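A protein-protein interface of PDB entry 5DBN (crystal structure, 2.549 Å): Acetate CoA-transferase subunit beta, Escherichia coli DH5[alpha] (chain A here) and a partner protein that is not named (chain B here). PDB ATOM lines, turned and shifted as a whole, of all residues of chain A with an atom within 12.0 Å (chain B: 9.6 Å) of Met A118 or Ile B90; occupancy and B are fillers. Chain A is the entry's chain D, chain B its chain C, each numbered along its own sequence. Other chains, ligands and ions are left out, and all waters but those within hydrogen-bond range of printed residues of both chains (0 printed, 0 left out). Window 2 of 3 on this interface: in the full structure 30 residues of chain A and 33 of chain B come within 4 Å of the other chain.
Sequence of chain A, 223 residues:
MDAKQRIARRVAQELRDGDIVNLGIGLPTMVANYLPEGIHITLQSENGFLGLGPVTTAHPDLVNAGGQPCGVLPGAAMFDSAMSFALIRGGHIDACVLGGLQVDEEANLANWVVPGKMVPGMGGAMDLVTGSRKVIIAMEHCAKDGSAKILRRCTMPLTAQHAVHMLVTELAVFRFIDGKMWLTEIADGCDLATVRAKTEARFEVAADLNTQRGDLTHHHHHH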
ATOM      1  N   LEU A 101     -35.131   8.145  -3.903  1.00  0.00           N
ATOM      2  CA  LEU A 101     -35.509   6.765  -3.639  1.00  0.00           C
ATOM      3  C   LEU A 101     -36.838   6.750  -2.898  1.00  0.00           C
ATOM      4  O   LEU A 101     -37.703   5.918  -3.172  1.00  0.00           O
ATOM      5  CB  LEU A 101     -34.434   6.051  -2.818  1.00  0.00           C
ATOM      6  CG  LEU A 101     -33.043   5.992  -3.446  1.00  0.00           C
ATOM      7  CD1 LEU A 101     -32.002   5.666  -2.390  1.00  0.00           C
ATOM      8  CD2 LEU A 101     -33.010   4.971  -4.571  1.00  0.00           C
ATOM      9  N   ASN A 111     -32.152   9.548  -0.705  1.00  0.00           N
ATOM     10  CA  ASN A 111     -31.634   9.417  -2.063  1.00  0.00           C
ATOM     11  C   ASN A 111     -30.113   9.278  -2.158  1.00  0.00           C
ATOM     12  O   ASN A 111     -29.525   9.662  -3.171  1.00  0.00           O
ATOM     13  CB  ASN A 111     -32.084  10.621  -2.900  1.00  0.00           C
ATOM     14  CG  ASN A 111     -31.280  11.880  -2.607  1.00  0.00           C
ATOM     15  OD1 ASN A 111     -30.768  12.065  -1.501  1.00  0.00           O
ATOM     16  ND2 ASN A 111     -31.164  12.749  -3.604  1.00  0.00           N
ATOM     17  N   TRP A 112     -29.477   8.733  -1.124  1.00  0.00           N
ATOM     18  CA  TRP A 112     -28.022   8.575  -1.143  1.00  0.00           C
ATOM     19  C   TRP A 112     -27.559   7.169  -0.765  1.00  0.00           C
ATOM     20  O   TRP A 112     -26.378   6.849  -0.901  1.00  0.00           O
ATOM     21  CB  TRP A 112     -27.364   9.592  -0.206  1.00  0.00           C
ATOM     22  CG  TRP A 112     -27.503   9.279   1.251  1.00  0.00           C
ATOM     23  CD1 TRP A 112     -28.581   9.531   2.048  1.00  0.00           C
ATOM     24  CD2 TRP A 112     -26.516   8.669   2.092  1.00  0.00           C
ATOM     25  NE1 TRP A 112     -28.329   9.109   3.332  1.00  0.00           N
ATOM     26  CE2 TRP A 112     -27.068   8.577   3.385  1.00  0.00           C
ATOM     27  CE3 TRP A 112     -25.220   8.189   1.877  1.00  0.00           C
ATOM     28  CZ2 TRP A 112     -26.370   8.023   4.457  1.00  0.00           C
ATOM     29  CZ3 TRP A 112     -24.529   7.641   2.943  1.00  0.00           C
ATOM     30  CH2 TRP A 112     -25.105   7.563   4.216  1.00  0.00           C
ATOM     31  N   VAL A 113     -28.477   6.330  -0.298  1.00  0.00           N
ATOM     32  CA  VAL A 113     -28.120   4.967   0.076  1.00  0.00           C
ATOM     33  C   VAL A 113     -29.334   4.041   0.097  1.00  0.00           C
ATOM     34  O   VAL A 113     -30.424   4.431   0.520  1.00  0.00           O
ATOM     35  CB  VAL A 113     -27.426   4.930   1.459  1.00  0.00           C
ATOM     36  CG1 VAL A 113     -28.332   5.518   2.535  1.00  0.00           C
ATOM     37  CG2 VAL A 113     -27.009   3.503   1.816  1.00  0.00           C
ATOM     38  N   VAL A 114     -29.129   2.818  -0.383  1.00  0.00           N
ATOM     39  CA  VAL A 114     -30.148   1.777  -0.335  1.00  0.00           C
ATOM     40  C   VAL A 114     -29.711   0.684   0.636  1.00  0.00           C
ATOM     41  O   VAL A 114     -28.633   0.109   0.472  1.00  0.00           O
ATOM     42  CB  VAL A 114     -30.388   1.152  -1.725  1.00  0.00           C
ATOM     43  CG1 VAL A 114     -31.461   0.068  -1.656  1.00  0.00           C
ATOM     44  CG2 VAL A 114     -30.771   2.223  -2.731  1.00  0.00           C
ATOM     45  N   PRO A 115     -30.538   0.391   1.655  1.00  0.00           N
ATOM     46  CA  PRO A 115     -30.156  -0.714   2.541  1.00  0.00           C
ATOM     47  C   PRO A 115     -30.103  -2.034   1.778  1.00  0.00           C
ATOM     48  O   PRO A 115     -31.047  -2.365   1.062  1.00  0.00           O
ATOM     49  CB  PRO A 115     -31.264  -0.719   3.602  1.00  0.00           C
ATOM     50  CG  PRO A 115     -32.422  -0.051   2.954  1.00  0.00           C
ATOM     51  CD  PRO A 115     -31.836   0.977   2.033  1.00  0.00           C
ATOM     52  N   GLY A 116     -29.009  -2.772   1.939  1.00  0.00           N
ATOM     53  CA  GLY A 116     -28.814  -4.020   1.225  1.00  0.00           C
ATOM     54  C   GLY A 116     -27.848  -3.842   0.068  1.00  0.00           C
ATOM     55  O   GLY A 116     -27.247  -4.811  -0.398  1.00  0.00           O
ATOM     56  N   LYS A 117     -27.698  -2.603  -0.394  1.00  0.00           N
ATOM     57  CA  LYS A 117     -26.710  -2.287  -1.419  1.00  0.00           C
ATOM     58  C   LYS A 117     -25.546  -1.567  -0.754  1.00  0.00           C
ATOM     59  O   LYS A 117     -25.705  -0.980   0.316  1.00  0.00           O
ATOM     60  CB  LYS A 117     -27.324  -1.423  -2.522  1.00  0.00           C
ATOM     61  N   MET A 118     -24.379  -1.603  -1.388  1.00  0.00           N
ATOM     62  CA  MET A 118     -23.192  -0.992  -0.805  1.00  0.00           C
ATOM     63  C   MET A 118     -23.346   0.530  -0.767  1.00  0.00           C
ATOM     64  O   MET A 118     -23.880   1.136  -1.696  1.00  0.00           O
ATOM     65  CB  MET A 118     -21.938  -1.435  -1.559  1.00  0.00           C
ATOM     66  CG  MET A 118     -20.645  -0.962  -0.920  1.00  0.00           C
ATOM     67  SD  MET A 118     -19.231  -2.006  -1.348  1.00  0.00           S
ATOM     68  CE  MET A 118     -19.019  -1.680  -3.093  1.00  0.00           C
ATOM     69  N   VAL A 119     -22.871   1.133   0.317  1.00  0.00           N
ATOM     70  CA  VAL A 119     -23.040   2.563   0.559  1.00  0.00           C
ATOM     71  C   VAL A 119     -22.035   3.414  -0.227  1.00  0.00           C
ATOM     72  O   VAL A 119     -20.826   3.247  -0.066  1.00  0.00           O
ATOM     73  CB  VAL A 119     -22.892   2.884   2.059  1.00  0.00           C
ATOM     74  CG1 VAL A 119     -23.326   4.313   2.344  1.00  0.00           C
ATOM     75  CG2 VAL A 119     -23.712   1.913   2.896  1.00  0.00           C
ATOM     76  N   PRO A 120     -22.533   4.325  -1.090  1.00  0.00           N
ATOM     77  CA  PRO A 120     -21.640   5.155  -1.908  1.00  0.00           C
ATOM     78  C   PRO A 120     -21.193   6.454  -1.236  1.00  0.00           C
ATOM     79  O   PRO A 120     -20.173   7.019  -1.633  1.00  0.00           O
ATOM     80  CB  PRO A 120     -22.500   5.469  -3.130  1.00  0.00           C
ATOM     81  CG  PRO A 120     -23.878   5.549  -2.580  1.00  0.00           C
ATOM     82  CD  PRO A 120     -23.947   4.555  -1.441  1.00  0.00           C
ATOM     83  N   GLY A 121     -21.945   6.913  -0.240  1.00  0.00           N
ATOM     84  CA  GLY A 121     -21.684   8.190   0.406  1.00  0.00           C
ATOM     85  C   GLY A 121     -22.719   9.208  -0.033  1.00  0.00           C
ATOM     86  O   GLY A 121     -23.384   9.009  -1.049  1.00  0.00           O
ATOM     87  N   MET A 122     -22.854  10.297   0.719  1.00  0.00           N
ATOM     88  CA  MET A 122     -23.901  11.280   0.449  1.00  0.00           C
ATOM     89  C   MET A 122     -23.450  12.372  -0.514  1.00  0.00           C
ATOM     90  O   MET A 122     -24.280  13.026  -1.148  1.00  0.00           O
ATOM     91  CB  MET A 122     -24.393  11.916   1.755  1.00  0.00           C
ATOM     92  CG  MET A 122     -23.348  12.714   2.534  1.00  0.00           C
ATOM     93  SD  MET A 122     -22.146  11.698   3.412  1.00  0.00           S
ATOM     94  CE  MET A 122     -23.188  10.894   4.630  1.00  0.00           C
ATOM     95  N   GLY A 123     -22.141  12.572  -0.621  1.00  0.00           N
ATOM     96  CA  GLY A 123     -21.604  13.629  -1.458  1.00  0.00           C
ATOM     97  C   GLY A 123     -22.083  15.000  -1.016  1.00  0.00           C
ATOM     98  O   GLY A 123     -21.926  15.370   0.148  1.00  0.00           O
ATOM     99  N   MET A 156     -35.854   4.237   4.397  1.00  0.00           N
ATOM    100  CA  MET A 156     -34.430   4.269   4.080  1.00  0.00           C
ATOM    101  C   MET A 156     -33.765   5.454   4.771  1.00  0.00           C
ATOM    102  O   MET A 156     -34.446   6.398   5.171  1.00  0.00           O
ATOM    103  CB  MET A 156     -34.213   4.345   2.568  1.00  0.00           C
ATOM    104  CG  MET A 156     -34.826   3.190   1.795  1.00  0.00           C
ATOM    105  SD  MET A 156     -34.493   3.281   0.025  1.00  0.00           S
ATOM    106  CE  MET A 156     -35.428   1.873  -0.564  1.00  0.00           C
ATOM    107  N   PRO A 157     -32.428   5.406   4.918  1.00  0.00           N
ATOM    108  CA  PRO A 157     -31.703   6.503   5.573  1.00  0.00           C
ATOM    109  C   PRO A 157     -31.956   7.845   4.904  1.00  0.00           C
ATOM    110  O   PRO A 157     -31.814   7.970   3.687  1.00  0.00           O
ATOM    111  CB  PRO A 157     -30.235   6.090   5.429  1.00  0.00           C
ATOM    112  CG  PRO A 157     -30.270   4.614   5.285  1.00  0.00           C
ATOM    113  CD  PRO A 157     -31.524   4.311   4.526  1.00  0.00           C
ATOM    114  N   HIS B  78     -17.634  10.700  -0.499  1.00  0.00           N
ATOM    115  CA  HIS B  78     -18.122   9.754  -1.500  1.00  0.00           C
ATOM    116  C   HIS B  78     -17.079   8.686  -1.821  1.00  0.00           C
ATOM    117  O   HIS B  78     -15.889   8.981  -1.918  1.00  0.00           O
ATOM    118  CB  HIS B  78     -18.524  10.496  -2.772  1.00  0.00           C
ATOM    119  CG  HIS B  78     -19.480   9.736  -3.636  1.00  0.00           C
ATOM    120  ND1 HIS B  78     -19.065   8.886  -4.638  1.00  0.00           N
ATOM    121  CD2 HIS B  78     -20.833   9.694  -3.643  1.00  0.00           C
ATOM    122  CE1 HIS B  78     -20.122   8.355  -5.228  1.00  0.00           C
ATOM    123  NE2 HIS B  78     -21.208   8.829  -4.642  1.00  0.00           N
ATOM    124  N   ILE B  79     -17.540   7.448  -1.989  1.00  0.00           N
ATOM    125  CA  ILE B  79     -16.653   6.315  -2.244  1.00  0.00           C
ATOM    126  C   ILE B  79     -17.224   5.358  -3.293  1.00  0.00           C
ATOM    127  O   ILE B  79     -16.707   4.256  -3.486  1.00  0.00           O
ATOM    128  CB  ILE B  79     -16.384   5.522  -0.950  1.00  0.00           C
ATOM    129  CG1 ILE B  79     -17.701   5.012  -0.350  1.00  0.00           C
ATOM    130  CG2 ILE B  79     -15.644   6.392   0.053  1.00  0.00           C
ATOM    131  CD1 ILE B  79     -17.521   4.021   0.782  1.00  0.00           C
ATOM    132  N   GLY B  80     -18.287   5.786  -3.967  1.00  0.00           N
ATOM    133  CA  GLY B  80     -19.029   4.919  -4.865  1.00  0.00           C
ATOM    134  C   GLY B  80     -18.261   4.446  -6.085  1.00  0.00           C
ATOM    135  O   GLY B  80     -18.453   3.318  -6.541  1.00  0.00           O
ATOM    136  N   THR B  81     -17.389   5.297  -6.619  1.00  0.00           N
ATOM    137  CA  THR B  81     -16.671   4.966  -7.847  1.00  0.00           C
ATOM    138  C   THR B  81     -15.444   4.094  -7.587  1.00  0.00           C
ATOM    139  O   THR B  81     -14.713   3.755  -8.520  1.00  0.00           O
ATOM    140  CB  THR B  81     -16.219   6.237  -8.593  1.00  0.00           C
ATOM    141  OG1 THR B  81     -15.472   7.081  -7.708  1.00  0.00           O
ATOM    142  CG2 THR B  81     -17.421   6.998  -9.132  1.00  0.00           C
ATOM    143  N   ASN B  82     -15.226   3.729  -6.325  1.00  0.00           N
ATOM    144  CA  ASN B  82     -14.143   2.821  -5.959  1.00  0.00           C
ATOM    145  C   ASN B  82     -14.669   1.650  -5.128  1.00  0.00           C
ATOM    146  O   ASN B  82     -14.806   1.765  -3.910  1.00  0.00           O
ATOM    147  CB  ASN B  82     -13.053   3.569  -5.188  1.00  0.00           C
ATOM    148  CG  ASN B  82     -11.747   2.800  -5.133  1.00  0.00           C
ATOM    149  OD1 ASN B  82     -11.723   1.580  -5.293  1.00  0.00           O
ATOM    150  ND2 ASN B  82     -10.649   3.516  -4.918  1.00  0.00           N
ATOM    151  N   PRO B  83     -14.978   0.517  -5.783  1.00  0.00           N
ATOM    152  CA  PRO B  83     -15.520  -0.630  -5.043  1.00  0.00           C
ATOM    153  C   PRO B  83     -14.562  -1.150  -3.973  1.00  0.00           C
ATOM    154  O   PRO B  83     -15.001  -1.757  -2.996  1.00  0.00           O
ATOM    155  CB  PRO B  83     -15.751  -1.680  -6.134  1.00  0.00           C
ATOM    156  CG  PRO B  83     -14.857  -1.284  -7.241  1.00  0.00           C
ATOM    157  CD  PRO B  83     -14.809   0.208  -7.213  1.00  0.00           C
ATOM    158  N   GLU B  84     -13.267  -0.914  -4.160  1.00  0.00           N
ATOM    159  CA  GLU B  84     -12.264  -1.385  -3.213  1.00  0.00           C
ATOM    160  C   GLU B  84     -12.460  -0.735  -1.853  1.00  0.00           C
ATOM    161  O   GLU B  84     -12.359  -1.395  -0.821  1.00  0.00           O
ATOM    162  CB  GLU B  84     -10.857  -1.087  -3.728  1.00  0.00           C
ATOM    163  CG  GLU B  84      -9.738  -1.678  -2.881  1.00  0.00           C
ATOM    164  CD  GLU B  84      -9.750  -3.191  -2.843  1.00  0.00           C
ATOM    165  OE1 GLU B  84     -10.385  -3.810  -3.724  1.00  0.00           O
ATOM    166  OE2 GLU B  84      -9.125  -3.762  -1.922  1.00  0.00           O
ATOM    167  N   THR B  85     -12.731   0.564  -1.861  1.00  0.00           N
ATOM    168  CA  THR B  85     -13.021   1.288  -0.633  1.00  0.00           C
ATOM    169  C   THR B  85     -14.193   0.647   0.105  1.00  0.00           C
ATOM    170  O   THR B  85     -14.111   0.382   1.306  1.00  0.00           O
ATOM    171  CB  THR B  85     -13.339   2.768  -0.916  1.00  0.00           C
ATOM    172  OG1 THR B  85     -12.245   3.371  -1.621  1.00  0.00           O
ATOM    173  CG2 THR B  85     -13.595   3.530   0.385  1.00  0.00           C
ATOM    174  N   GLY B  86     -15.278   0.394  -0.621  1.00  0.00           N
ATOM    175  CA  GLY B  86     -16.463  -0.213  -0.041  1.00  0.00           C
ATOM    176  C   GLY B  86     -16.230  -1.595   0.541  1.00  0.00           C
ATOM    177  O   GLY B  86     -16.683  -1.894   1.643  1.00  0.00           O
ATOM    178  N   ARG B  87     -15.548  -2.452  -0.208  1.00  0.00           N
ATOM    179  CA  ARG B  87     -15.236  -3.796   0.268  1.00  0.00           C
ATOM    180  C   ARG B  87     -14.384  -3.779   1.537  1.00  0.00           C
ATOM    181  O   ARG B  87     -14.676  -4.507   2.486  1.00  0.00           O
ATOM    182  CB  ARG B  87     -14.568  -4.601  -0.843  1.00  0.00           C
ATOM    183  CG  ARG B  87     -14.394  -6.073  -0.528  1.00  0.00           C
ATOM    184  CD  ARG B  87     -13.530  -6.723  -1.584  1.00  0.00           C
ATOM    185  NE  ARG B  87     -12.149  -6.253  -1.591  1.00  0.00           N
ATOM    186  CZ  ARG B  87     -11.292  -6.511  -2.575  1.00  0.00           C
ATOM    187  NH1 ARG B  87     -11.691  -7.203  -3.635  1.00  0.00           N
ATOM    188  NH2 ARG B  87     -10.049  -6.056  -2.517  1.00  0.00           N
ATOM    189  N   ARG B  88     -13.337  -2.961   1.558  1.00  0.00           N
ATOM    190  CA  ARG B  88     -12.479  -2.880   2.736  1.00  0.00           C
ATOM    191  C   ARG B  88     -13.262  -2.244   3.890  1.00  0.00           C
ATOM    192  O   ARG B  88     -12.989  -2.518   5.057  1.00  0.00           O
ATOM    193  CB  ARG B  88     -11.194  -2.093   2.439  1.00  0.00           C
ATOM    194  CG  ARG B  88     -10.350  -2.691   1.314  1.00  0.00           C
ATOM    195  CD  ARG B  88      -9.086  -1.885   1.040  1.00  0.00           C
ATOM    196  NE  ARG B  88      -8.015  -2.248   1.965  1.00  0.00           N
ATOM    197  CZ  ARG B  88      -7.165  -3.254   1.775  1.00  0.00           C
ATOM    198  NH1 ARG B  88      -7.244  -4.007   0.685  1.00  0.00           N
ATOM    199  NH2 ARG B  88      -6.227  -3.507   2.677  1.00  0.00           N
ATOM    200  N   MET B  89     -14.233  -1.396   3.558  1.00  0.00           N
ATOM    201  CA  MET B  89     -15.130  -0.825   4.562  1.00  0.00           C
ATOM    202  C   MET B  89     -16.016  -1.904   5.181  1.00  0.00           C
ATOM    203  O   MET B  89     -16.131  -2.004   6.403  1.00  0.00           O
ATOM    204  CB  MET B  89     -16.003   0.270   3.945  1.00  0.00           C
ATOM    205  CG  MET B  89     -16.946   0.955   4.927  1.00  0.00           C
ATOM    206  SD  MET B  89     -17.936   2.243   4.141  1.00  0.00           S
ATOM    207  CE  MET B  89     -18.734   2.984   5.561  1.00  0.00           C
ATOM    208  N   ILE B  90     -16.639  -2.710   4.326  1.00  0.00           N
ATOM    209  CA  ILE B  90     -17.526  -3.781   4.772  1.00  0.00           C
ATOM    210  C   ILE B  90     -16.757  -4.857   5.532  1.00  0.00           C
ATOM    211  O   ILE B  90     -17.183  -5.299   6.598  1.00  0.00           O
ATOM    212  CB  ILE B  90     -18.269  -4.427   3.577  1.00  0.00           C
ATOM    213  CG1 ILE B  90     -19.200  -3.408   2.917  1.00  0.00           C
ATOM    214  CG2 ILE B  90     -19.079  -5.642   4.025  1.00  0.00           C
ATOM    215  CD1 ILE B  90     -19.719  -3.833   1.554  1.00  0.00           C
ATOM    216  N   SER B  91     -15.629  -5.281   4.969  1.00  0.00           N
ATOM    217  CA  SER B  91     -14.830  -6.352   5.554  1.00  0.00           C
ATOM    218  C   SER B  91     -14.358  -5.979   6.956  1.00  0.00           C
ATOM    219  O   SER B  91     -14.368  -6.810   7.861  1.00  0.00           O
ATOM    220  CB  SER B  91     -13.630  -6.679   4.664  1.00  0.00           C
ATOM    221  OG  SER B  91     -12.683  -5.628   4.673  1.00  0.00           O
ATOM    222  N   GLY B  92     -13.925  -4.732   7.117  1.00  0.00           N
ATOM    223  CA  GLY B  92     -13.432  -4.241   8.392  1.00  0.00           C
ATOM    224  C   GLY B  92     -11.968  -3.853   8.328  1.00  0.00           C
ATOM    225  O   GLY B  92     -11.424  -3.298   9.282  1.00  0.00           O
ATOM    226  N   GLU B  93     -11.331  -4.147   7.197  1.00  0.00           N
ATOM    227  CA  GLU B  93      -9.915  -3.851   6.995  1.00  0.00           C
ATOM    228  C   GLU B  93      -9.636  -2.351   7.042  1.00  0.00           C
ATOM    229  O   GLU B  93      -8.516  -1.931   7.328  1.00  0.00           O
ATOM    230  CB  GLU B  93      -9.440  -4.420   5.657  1.00  0.00           C
ATOM    231  CG  GLU B  93      -9.528  -5.938   5.561  1.00  0.00           C
ATOM    232  CD  GLU B  93      -9.208  -6.455   4.173  1.00  0.00           C
ATOM    233  OE1 GLU B  93      -9.742  -7.521   3.796  1.00  0.00           O
ATOM    234  OE2 GLU B  93      -8.420  -5.800   3.459  1.00  0.00           O
ATOM    235  N   MET B  94     -10.663  -1.554   6.769  1.00  0.00           N
ATOM    236  CA  MET B  94     -10.517  -0.107   6.675  1.00  0.00           C
ATOM    237  C   MET B  94     -11.676   0.624   7.337  1.00  0.00           C
ATOM    238  O   MET B  94     -12.837   0.258   7.166  1.00  0.00           O
ATOM    239  CB  MET B  94     -10.418   0.310   5.205  1.00  0.00           C
ATOM    240  CG  MET B  94     -10.227   1.805   4.984  1.00  0.00           C
ATOM    241  SD  MET B  94      -9.877   2.236   3.265  1.00  0.00           S
ATOM    242  CE  MET B  94      -8.212   1.625   3.137  1.00  0.00           C
ATOM    243  N   ASP B  95     -11.344   1.663   8.095  1.00  0.00           N
ATOM    244  CA  ASP B  95     -12.349   2.501   8.728  1.00  0.00           C
ATOM    245  C   ASP B  95     -12.703   3.617   7.757  1.00  0.00           C
ATOM    246  O   ASP B  95     -11.817   4.199   7.137  1.00  0.00           O
ATOM    247  CB  ASP B  95     -11.824   3.069  10.050  1.00  0.00           C
ATOM    248  CG  ASP B  95     -12.876   3.851  10.811  1.00  0.00           C
ATOM    249  OD1 ASP B  95     -14.071   3.498  10.714  1.00  0.00           O
ATOM    250  OD2 ASP B  95     -12.506   4.821  11.508  1.00  0.00           O
ATOM    251  N   VAL B  96     -13.992   3.911   7.617  1.00  0.00           N
ATOM    252  CA  VAL B  96     -14.435   4.940   6.681  1.00  0.00           C
ATOM    253  C   VAL B  96     -15.413   5.891   7.353  1.00  0.00           C
ATOM    254  O   VAL B  96     -16.422   5.464   7.911  1.00  0.00           O
ATOM    255  CB  VAL B  96     -15.093   4.321   5.434  1.00  0.00           C
ATOM    256  CG1 VAL B  96     -15.511   5.412   4.448  1.00  0.00           C
ATOM    257  CG2 VAL B  96     -14.142   3.338   4.769  1.00  0.00           C
ATOM    258  N   LEU B  98     -17.867   8.821   6.449  1.00  0.00           N
ATOM    259  CA  LEU B  98     -18.582   9.520   5.393  1.00  0.00           C
ATOM    260  C   LEU B  98     -19.180  10.818   5.925  1.00  0.00           C
ATOM    261  O   LEU B  98     -20.086  10.801   6.760  1.00  0.00           O
ATOM    262  CB  LEU B  98     -19.668   8.616   4.808  1.00  0.00           C
ATOM    263  CG  LEU B  98     -19.114   7.335   4.178  1.00  0.00           C
ATOM    264  CD1 LEU B  98     -20.243   6.373   3.851  1.00  0.00           C
ATOM    265  CD2 LEU B  98     -18.311   7.645   2.924  1.00  0.00           C
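The backbone NH of Gly B80 lies within hydrogen-bond range of the backbone carbonyl oxygen of Pro A120 (3.2 Å).
N of Ile B79 is in hydrogen-bond range of O of Pro A120 (2.7 Å).
N of Gly B80 is in hydrogen-bond range of ND1 of His B78.
The backbone carbonyl oxygen of Arg B87 is in hydrogen-bond range of the side-chain hydroxyl of Ser B91 (3.2 Å).
The guanidinium group (NH2) of Arg B87 lies within salt-bridge range of the side-chain carboxylate (OE2) of Glu B84, at 2.5 Å.
Of the 20 printed residues of chain B, 7 touch a printed residue of chain A.
Hydrophobic or aromatic side chains of chain B that line the printed part of chain A: His B78, Ile B79 and Ile B90.
Of the 16 printed residues of chain A, 5 touch a printed residue of chain B.
Printed residues of chain A that touch a printed residue of chain B: Met A118, Val A119, Pro A120, Gly A121 and Met A122.
Among the printed residues, merely in contact across the chains: Pro A120 with His B78, Met A118 with Ile B90, Val A119 with Ile B79, Met A118 with Gly B86, Gly A121 with His B78, Met A122 with Leu B98 and Met A118 with Arg B87.
Pro A115 touches none of the printed residues of chain B.
No residue of chain B comes within 4 Å of Lys A117.
Printed residues of chain B within 4 Å of Met A118: Gly B86, Arg B87 and Ile B90.
Of the printed residues of chain A, His B78 touches Pro A120 and Gly A121.
Of the printed residues of chain A, Ile B79 touches Val A119 and Pro A120.
Gly B80 touches just one residue of chain A: Pro A120.
Of chain A, only Met A118 (3.5 Å) comes within 4 Å of Gly B86.
Printed residues of chain A within 4 Å of Arg B87: Met A118.
No residue of chain A comes within 4 Å of Met B89.
Of chain A, only Met A118 comes within 4 Å of Ile B90.
No residue of chain A comes within 4 Å of Ser B91.
No residue of chain A comes within 4 Å of Gly B92.
Of the printed residues of chain A, Leu B98 touches Met A122.
The nearest printed residue of chain B that does not touch Met A118 is Pro B83 (4.02 Å).
The nearest printed residue of chain A that does not touch Ile B79 is Gly A121 (4.7 Å).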
